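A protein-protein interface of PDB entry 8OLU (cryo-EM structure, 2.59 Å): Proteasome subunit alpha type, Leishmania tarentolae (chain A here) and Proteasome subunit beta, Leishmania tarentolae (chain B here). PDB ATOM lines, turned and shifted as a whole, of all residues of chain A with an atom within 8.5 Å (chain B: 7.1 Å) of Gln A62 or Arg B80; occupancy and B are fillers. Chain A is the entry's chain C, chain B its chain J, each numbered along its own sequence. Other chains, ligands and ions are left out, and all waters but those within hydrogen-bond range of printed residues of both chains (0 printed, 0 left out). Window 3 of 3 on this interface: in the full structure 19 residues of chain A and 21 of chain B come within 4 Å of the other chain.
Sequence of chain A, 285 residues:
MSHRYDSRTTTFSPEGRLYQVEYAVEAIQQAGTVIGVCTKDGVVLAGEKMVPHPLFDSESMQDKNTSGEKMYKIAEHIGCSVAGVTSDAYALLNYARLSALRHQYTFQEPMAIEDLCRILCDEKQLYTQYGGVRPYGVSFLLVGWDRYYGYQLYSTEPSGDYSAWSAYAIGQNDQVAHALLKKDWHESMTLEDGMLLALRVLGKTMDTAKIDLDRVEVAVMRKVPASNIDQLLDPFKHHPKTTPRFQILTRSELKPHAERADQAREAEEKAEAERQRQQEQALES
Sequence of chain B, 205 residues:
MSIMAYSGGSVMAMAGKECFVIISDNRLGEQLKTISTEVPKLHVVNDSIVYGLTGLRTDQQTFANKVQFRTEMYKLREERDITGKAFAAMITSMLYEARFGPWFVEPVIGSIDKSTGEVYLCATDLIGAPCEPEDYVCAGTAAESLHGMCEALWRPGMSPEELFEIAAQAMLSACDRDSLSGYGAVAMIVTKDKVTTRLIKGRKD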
ATOM      1  N   GLU A  59     -21.377 -11.169   3.194  1.00  0.00           N
ATOM      2  CA  GLU A  59     -21.469 -12.345   4.039  1.00  0.00           C
ATOM      3  C   GLU A  59     -20.412 -12.320   5.165  1.00  0.00           C
ATOM      4  O   GLU A  59     -20.367 -13.262   5.964  1.00  0.00           O
ATOM      5  CB  GLU A  59     -21.346 -13.599   3.162  1.00  0.00           C
ATOM      6  CG  GLU A  59     -22.440 -13.791   2.111  1.00  0.00           C
ATOM      7  CD  GLU A  59     -22.483 -15.195   1.484  1.00  0.00           C
ATOM      8  OE1 GLU A  59     -22.496 -15.303   0.196  1.00  0.00           O
ATOM      9  OE2 GLU A  59     -22.502 -16.198   2.273  1.00  0.00           O
ATOM     10  N   SER A  60     -19.519 -11.309   5.168  1.00  0.00           N
ATOM     11  CA  SER A  60     -18.376 -11.190   6.072  1.00  0.00           C
ATOM     12  C   SER A  60     -17.564 -12.485   6.178  1.00  0.00           C
ATOM     13  O   SER A  60     -17.246 -12.956   7.269  1.00  0.00           O
ATOM     14  CB  SER A  60     -18.813 -10.701   7.458  1.00  0.00           C
ATOM     15  OG  SER A  60     -19.151  -9.303   7.445  1.00  0.00           O
ATOM     16  N   MET A  61     -17.172 -13.058   5.054  1.00  0.00           N
ATOM     17  CA  MET A  61     -16.372 -14.269   5.101  1.00  0.00           C
ATOM     18  C   MET A  61     -14.957 -13.884   5.531  1.00  0.00           C
ATOM     19  O   MET A  61     -14.523 -12.748   5.305  1.00  0.00           O
ATOM     20  CB  MET A  61     -16.326 -14.951   3.730  1.00  0.00           C
ATOM     21  CG  MET A  61     -17.710 -15.399   3.222  1.00  0.00           C
ATOM     22  SD  MET A  61     -18.604 -16.712   4.160  1.00  0.00           S
ATOM     23  CE  MET A  61     -19.098 -17.740   2.770  1.00  0.00           C
ATOM     24  N   GLN A  62     -14.266 -14.827   6.177  1.00  0.00           N
ATOM     25  CA  GLN A  62     -12.977 -14.564   6.774  1.00  0.00           C
ATOM     26  C   GLN A  62     -11.914 -14.605   5.672  1.00  0.00           C
ATOM     27  O   GLN A  62     -10.981 -13.807   5.690  1.00  0.00           O
ATOM     28  CB  GLN A  62     -12.815 -15.521   7.950  1.00  0.00           C
ATOM     29  CG  GLN A  62     -11.464 -15.437   8.669  1.00  0.00           C
ATOM     30  CD  GLN A  62     -11.279 -16.580   9.653  1.00  0.00           C
ATOM     31  OE1 GLN A  62     -11.938 -16.620  10.699  1.00  0.00           O
ATOM     32  NE2 GLN A  62     -10.402 -17.525   9.312  1.00  0.00           N
ATOM     33  N   ASP A  63     -12.122 -15.457   4.651  1.00  0.00           N
ATOM     34  CA  ASP A  63     -11.240 -15.566   3.493  1.00  0.00           C
ATOM     35  C   ASP A  63     -11.849 -14.838   2.306  1.00  0.00           C
ATOM     36  O   ASP A  63     -12.865 -15.255   1.749  1.00  0.00           O
ATOM     37  CB  ASP A  63     -11.011 -17.006   3.024  1.00  0.00           C
ATOM     38  CG  ASP A  63     -10.266 -17.922   3.985  1.00  0.00           C
ATOM     39  OD1 ASP A  63     -10.344 -19.171   3.764  1.00  0.00           O
ATOM     40  OD2 ASP A  63      -9.603 -17.398   4.936  1.00  0.00           O
ATOM     41  N   LYS A  64     -11.167 -13.766   1.902  1.00  0.00           N
ATOM     42  CA  LYS A  64     -11.720 -12.805   0.969  1.00  0.00           C
ATOM     43  C   LYS A  64     -11.573 -13.339  -0.450  1.00  0.00           C
ATOM     44  O   LYS A  64     -12.432 -13.079  -1.286  1.00  0.00           O
ATOM     45  CB  LYS A  64     -11.072 -11.451   1.277  1.00  0.00           C
ATOM     46  CG  LYS A  64     -11.575 -10.815   2.572  1.00  0.00           C
ATOM     47  CD  LYS A  64     -13.089 -10.592   2.509  1.00  0.00           C
ATOM     48  CE  LYS A  64     -13.614  -9.413   3.311  1.00  0.00           C
ATOM     49  NZ  LYS A  64     -13.938  -9.803   4.704  1.00  0.00           N
ATOM     50  N   ASN A  65     -10.587 -14.212  -0.664  1.00  0.00           N
ATOM     51  CA  ASN A  65     -10.229 -14.691  -1.991  1.00  0.00           C
ATOM     52  C   ASN A  65     -10.939 -15.974  -2.421  1.00  0.00           C
ATOM     53  O   ASN A  65     -10.769 -16.410  -3.550  1.00  0.00           O
ATOM     54  CB  ASN A  65      -8.719 -14.926  -2.095  1.00  0.00           C
ATOM     55  CG  ASN A  65      -7.939 -13.660  -1.829  1.00  0.00           C
ATOM     56  OD1 ASN A  65      -8.246 -12.592  -2.360  1.00  0.00           O
ATOM     57  ND2 ASN A  65      -6.963 -13.771  -0.947  1.00  0.00           N
ATOM     58  N   THR A  66     -11.751 -16.588  -1.581  1.00  0.00           N
ATOM     59  CA  THR A  66     -12.320 -17.854  -1.985  1.00  0.00           C
ATOM     60  C   THR A  66     -13.572 -17.648  -2.836  1.00  0.00           C
ATOM     61  O   THR A  66     -13.904 -18.484  -3.673  1.00  0.00           O
ATOM     62  CB  THR A  66     -12.612 -18.743  -0.769  1.00  0.00           C
ATOM     63  OG1 THR A  66     -11.456 -18.864   0.058  1.00  0.00           O
ATOM     64  CG2 THR A  66     -12.995 -20.152  -1.157  1.00  0.00           C
ATOM     65  N   ASN B  46      -2.944 -25.717   9.357  1.00  0.00           N
ATOM     66  CA  ASN B  46      -3.021 -24.286   9.143  1.00  0.00           C
ATOM     67  C   ASN B  46      -2.168 -23.664  10.236  1.00  0.00           C
ATOM     68  O   ASN B  46      -1.682 -24.371  11.094  1.00  0.00           O
ATOM     69  CB  ASN B  46      -4.463 -23.726   9.144  1.00  0.00           C
ATOM     70  CG  ASN B  46      -5.281 -23.980  10.407  1.00  0.00           C
ATOM     71  OD1 ASN B  46      -4.796 -23.898  11.534  1.00  0.00           O
ATOM     72  ND2 ASN B  46      -6.556 -24.293  10.243  1.00  0.00           N
ATOM     73  N   THR B  71     -10.021 -31.063   5.137  1.00  0.00           N
ATOM     74  CA  THR B  71      -9.724 -29.732   5.574  1.00  0.00           C
ATOM     75  C   THR B  71      -9.677 -28.746   4.445  1.00  0.00           C
ATOM     76  O   THR B  71      -9.942 -27.605   4.702  1.00  0.00           O
ATOM     77  CB  THR B  71      -8.398 -29.605   6.313  1.00  0.00           C
ATOM     78  OG1 THR B  71      -7.315 -30.144   5.561  1.00  0.00           O
ATOM     79  CG2 THR B  71      -8.487 -30.310   7.639  1.00  0.00           C
ATOM     80  N   TYR B  74     -13.299 -28.044   3.511  1.00  0.00           N
ATOM     81  CA  TYR B  74     -13.786 -27.178   4.542  1.00  0.00           C
ATOM     82  C   TYR B  74     -13.441 -25.750   4.269  1.00  0.00           C
ATOM     83  O   TYR B  74     -14.290 -24.915   4.345  1.00  0.00           O
ATOM     84  CB  TYR B  74     -13.116 -27.531   5.849  1.00  0.00           C
ATOM     85  CG  TYR B  74     -13.656 -26.818   7.046  1.00  0.00           C
ATOM     86  CD1 TYR B  74     -13.195 -25.572   7.424  1.00  0.00           C
ATOM     87  CD2 TYR B  74     -14.669 -27.372   7.785  1.00  0.00           C
ATOM     88  CE1 TYR B  74     -13.726 -24.884   8.490  1.00  0.00           C
ATOM     89  CE2 TYR B  74     -15.188 -26.710   8.882  1.00  0.00           C
ATOM     90  CZ  TYR B  74     -14.719 -25.462   9.225  1.00  0.00           C
ATOM     91  OH  TYR B  74     -15.207 -24.875  10.362  1.00  0.00           O
ATOM     92  N   LYS B  75     -12.207 -25.493   3.959  1.00  0.00           N
ATOM     93  CA  LYS B  75     -11.702 -24.150   3.798  1.00  0.00           C
ATOM     94  C   LYS B  75     -12.289 -23.521   2.549  1.00  0.00           C
ATOM     95  O   LYS B  75     -12.488 -22.325   2.505  1.00  0.00           O
ATOM     96  CB  LYS B  75     -10.177 -24.288   3.874  1.00  0.00           C
ATOM     97  CG  LYS B  75      -9.358 -23.220   3.218  1.00  0.00           C
ATOM     98  CD  LYS B  75      -8.709 -22.313   4.180  1.00  0.00           C
ATOM     99  CE  LYS B  75      -7.935 -21.210   3.491  1.00  0.00           C
ATOM    100  NZ  LYS B  75      -7.866 -20.015   4.373  1.00  0.00           N
ATOM    101  N   LEU B  76     -12.610 -24.297   1.536  1.00  0.00           N
ATOM    102  CA  LEU B  76     -13.272 -23.713   0.391  1.00  0.00           C
ATOM    103  C   LEU B  76     -14.740 -23.426   0.649  1.00  0.00           C
ATOM    104  O   LEU B  76     -15.256 -22.401   0.246  1.00  0.00           O
ATOM    105  CB  LEU B  76     -13.203 -24.682  -0.775  1.00  0.00           C
ATOM    106  CG  LEU B  76     -11.836 -24.794  -1.432  1.00  0.00           C
ATOM    107  CD1 LEU B  76     -11.722 -26.070  -2.237  1.00  0.00           C
ATOM    108  CD2 LEU B  76     -11.561 -23.634  -2.320  1.00  0.00           C
ATOM    109  N   ARG B  77     -15.462 -24.410   1.162  1.00  0.00           N
ATOM    110  CA  ARG B  77     -16.861 -24.220   1.429  1.00  0.00           C
ATOM    111  C   ARG B  77     -17.074 -23.085   2.421  1.00  0.00           C
ATOM    112  O   ARG B  77     -17.981 -22.278   2.286  1.00  0.00           O
ATOM    113  CB  ARG B  77     -17.447 -25.443   2.085  1.00  0.00           C
ATOM    114  CG  ARG B  77     -17.686 -26.611   1.175  1.00  0.00           C
ATOM    115  CD  ARG B  77     -18.580 -27.570   1.958  1.00  0.00           C
ATOM    116  NE  ARG B  77     -18.946 -28.642   1.031  1.00  0.00           N
ATOM    117  CZ  ARG B  77     -18.353 -29.842   1.035  1.00  0.00           C
ATOM    118  NH1 ARG B  77     -17.625 -30.211   2.088  1.00  0.00           N
ATOM    119  NH2 ARG B  77     -18.511 -30.668   0.006  1.00  0.00           N
ATOM    120  N   GLU B  78     -16.278 -23.061   3.456  1.00  0.00           N
ATOM    121  CA  GLU B  78     -16.535 -22.231   4.589  1.00  0.00           C
ATOM    122  C   GLU B  78     -15.782 -20.928   4.506  1.00  0.00           C
ATOM    123  O   GLU B  78     -16.088 -20.002   5.246  1.00  0.00           O
ATOM    124  CB  GLU B  78     -16.042 -22.912   5.861  1.00  0.00           C
ATOM    125  CG  GLU B  78     -16.817 -24.180   6.220  1.00  0.00           C
ATOM    126  CD  GLU B  78     -17.316 -24.329   7.670  1.00  0.00           C
ATOM    127  OE1 GLU B  78     -17.996 -25.361   7.931  1.00  0.00           O
ATOM    128  OE2 GLU B  78     -17.062 -23.426   8.547  1.00  0.00           O
ATOM    129  N   GLU B  79     -14.769 -20.853   3.671  1.00  0.00           N
ATOM    130  CA  GLU B  79     -14.020 -19.613   3.532  1.00  0.00           C
ATOM    131  C   GLU B  79     -13.474 -19.227   4.890  1.00  0.00           C
ATOM    132  O   GLU B  79     -13.463 -18.095   5.262  1.00  0.00           O
ATOM    133  CB  GLU B  79     -14.836 -18.526   2.853  1.00  0.00           C
ATOM    134  CG  GLU B  79     -15.604 -19.098   1.699  1.00  0.00           C
ATOM    135  CD  GLU B  79     -16.150 -18.237   0.559  1.00  0.00           C
ATOM    136  OE1 GLU B  79     -16.658 -18.882  -0.459  1.00  0.00           O
ATOM    137  OE2 GLU B  79     -16.139 -16.942   0.668  1.00  0.00           O
ATOM    138  N   ARG B  80     -12.971 -20.190   5.624  1.00  0.00           N
ATOM    139  CA  ARG B  80     -12.149 -19.840   6.749  1.00  0.00           C
ATOM    140  C   ARG B  80     -11.328 -21.073   7.116  1.00  0.00           C
ATOM    141  O   ARG B  80     -11.535 -22.142   6.597  1.00  0.00           O
ATOM    142  CB  ARG B  80     -12.999 -19.424   7.946  1.00  0.00           C
ATOM    143  CG  ARG B  80     -14.012 -20.477   8.384  1.00  0.00           C
ATOM    144  CD  ARG B  80     -14.668 -20.221   9.736  1.00  0.00           C
ATOM    145  NE  ARG B  80     -15.706 -21.228   9.980  1.00  0.00           N
ATOM    146  CZ  ARG B  80     -16.145 -21.617  11.176  1.00  0.00           C
ATOM    147  NH1 ARG B  80     -15.713 -20.997  12.257  1.00  0.00           N
ATOM    148  NH2 ARG B  80     -17.010 -22.624  11.294  1.00  0.00           N
ATOM    149  N   ASP B  81     -10.369 -20.890   7.995  1.00  0.00           N
ATOM    150  CA  ASP B  81      -9.589 -21.991   8.452  1.00  0.00           C
ATOM    151  C   ASP B  81     -10.390 -22.756   9.486  1.00  0.00           C
ATOM    152  O   ASP B  81     -10.972 -22.150  10.381  1.00  0.00           O
ATOM    153  CB  ASP B  81      -8.304 -21.485   9.111  1.00  0.00           C
ATOM    154  CG  ASP B  81      -7.180 -21.117   8.142  1.00  0.00           C
ATOM    155  OD1 ASP B  81      -7.031 -21.841   7.066  1.00  0.00           O
ATOM    156  OD2 ASP B  81      -6.399 -20.140   8.500  1.00  0.00           O
ATOM    157  N   ILE B  82     -10.304 -24.075   9.442  1.00  0.00           N
ATOM    158  CA  ILE B  82     -10.834 -24.860  10.525  1.00  0.00           C
ATOM    159  C   ILE B  82     -10.110 -24.512  11.792  1.00  0.00           C
ATOM    160  O   ILE B  82      -8.980 -24.043  11.728  1.00  0.00           O
ATOM    161  CB  ILE B  82     -10.770 -26.351  10.203  1.00  0.00           C
ATOM    162  CG1 ILE B  82     -11.687 -27.157  11.118  1.00  0.00           C
ATOM    163  CG2 ILE B  82      -9.360 -26.885  10.190  1.00  0.00           C
ATOM    164  CD1 ILE B  82     -12.218 -28.421  10.459  1.00  0.00           C
ATOM    165  N   THR B  83     -10.788 -24.646  12.925  1.00  0.00           N
ATOM    166  CA  THR B  83     -10.191 -24.406  14.231  1.00  0.00           C
ATOM    167  C   THR B  83      -9.931 -25.719  14.915  1.00  0.00           C
ATOM    168  O   THR B  83     -10.571 -26.707  14.605  1.00  0.00           O
ATOM    169  CB  THR B  83     -11.162 -23.777  15.229  1.00  0.00           C
ATOM    170  OG1 THR B  83     -12.159 -24.728  15.626  1.00  0.00           O
ATOM    171  CG2 THR B  83     -11.873 -22.596  14.636  1.00  0.00           C
ATOM    172  N   ALA B  86     -13.057 -27.828  16.013  1.00  0.00           N
ATOM    173  CA  ALA B  86     -13.736 -28.430  14.885  1.00  0.00           C
ATOM    174  C   ALA B  86     -12.888 -29.531  14.301  1.00  0.00           C
ATOM    175  O   ALA B  86     -13.396 -30.600  13.962  1.00  0.00           O
ATOM    176  CB  ALA B  86     -13.977 -27.420  13.842  1.00  0.00           C
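The side-chain amino group (NZ) of Lys B75 is in salt-bridge range of the side-chain carboxylate (OD1) of Asp A63 (2.7 Å). N of Asp A63 lies within hydrogen-bond range of O of Glu B79 (3.0 Å). O of Glu B79 lies within hydrogen-bond range of N of Gln A62, 3.5 Å away. The backbone NH (N) of Arg B80 lies within hydrogen-bond range of the side-chain carboxylate (OD1) of Asp A63 (3.4 Å).
The side-chain amino group (NZ) of Lys A64 is in hydrogen-bond range of the backbone carbonyl oxygen (O) of Met A61. OD1 of Asp B81 is in salt-bridge range of NZ of Lys B75. NH2 of Arg B80 is in salt-bridge range of OE2 of Glu B78 (2.9 Å). NH2 of Arg B80 lies within hydrogen-bond range of OH of Tyr B74, 3.0 Å away.
Met A61 touches Glu B79. Gln A62 touches Arg B80 (NE2 to CB, 3.5 Å). N of Asp B81 touches NE2 of Gln A62, 3.6 Å away. CG2 of Thr A66 touches O of Leu B76, 3.5 Å away. CD of Glu B79 touches CB of Thr A66, at 3.8 Å.
Of chain B, only Glu B79 (3.5 Å), Arg B80 (3.5 Å) and Asp B81 (3.6 Å) come within 4 Å of Gln A62. Of chain A, only Gln A62 (3.5 Å) and Asp A63 (3.4 Å) come within 4 Å of Arg B80. Printed residues of chain A within 4 Å of Lys B75: Asp A63. Printed residues of chain A within 4 Å of Asp B81: Gln A62. Of the printed residues of chain B, Met A61 touches Glu B79 (3.4 Å). Of the printed residues of chain B, Thr A66 touches Leu B76 and Glu B79. Of the printed residues of chain A, Leu B76 touches Thr A66 (3.5 Å). The nearest residue of chain A that does not touch Arg B80 is Thr A66 (5.9 Å). The nearest printed residue of chain B that does not touch Thr A66 is Lys B75 (4.3 Å).
Of the 8 printed residues of chain A, 4 touch a printed residue of chain B. Hydrophobic or aromatic side chains of chain A within 4 Å of the printed part of chain B: Met A61. Along chain A the printed residues that touch a printed residue of chain B span positions 61 to 66.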
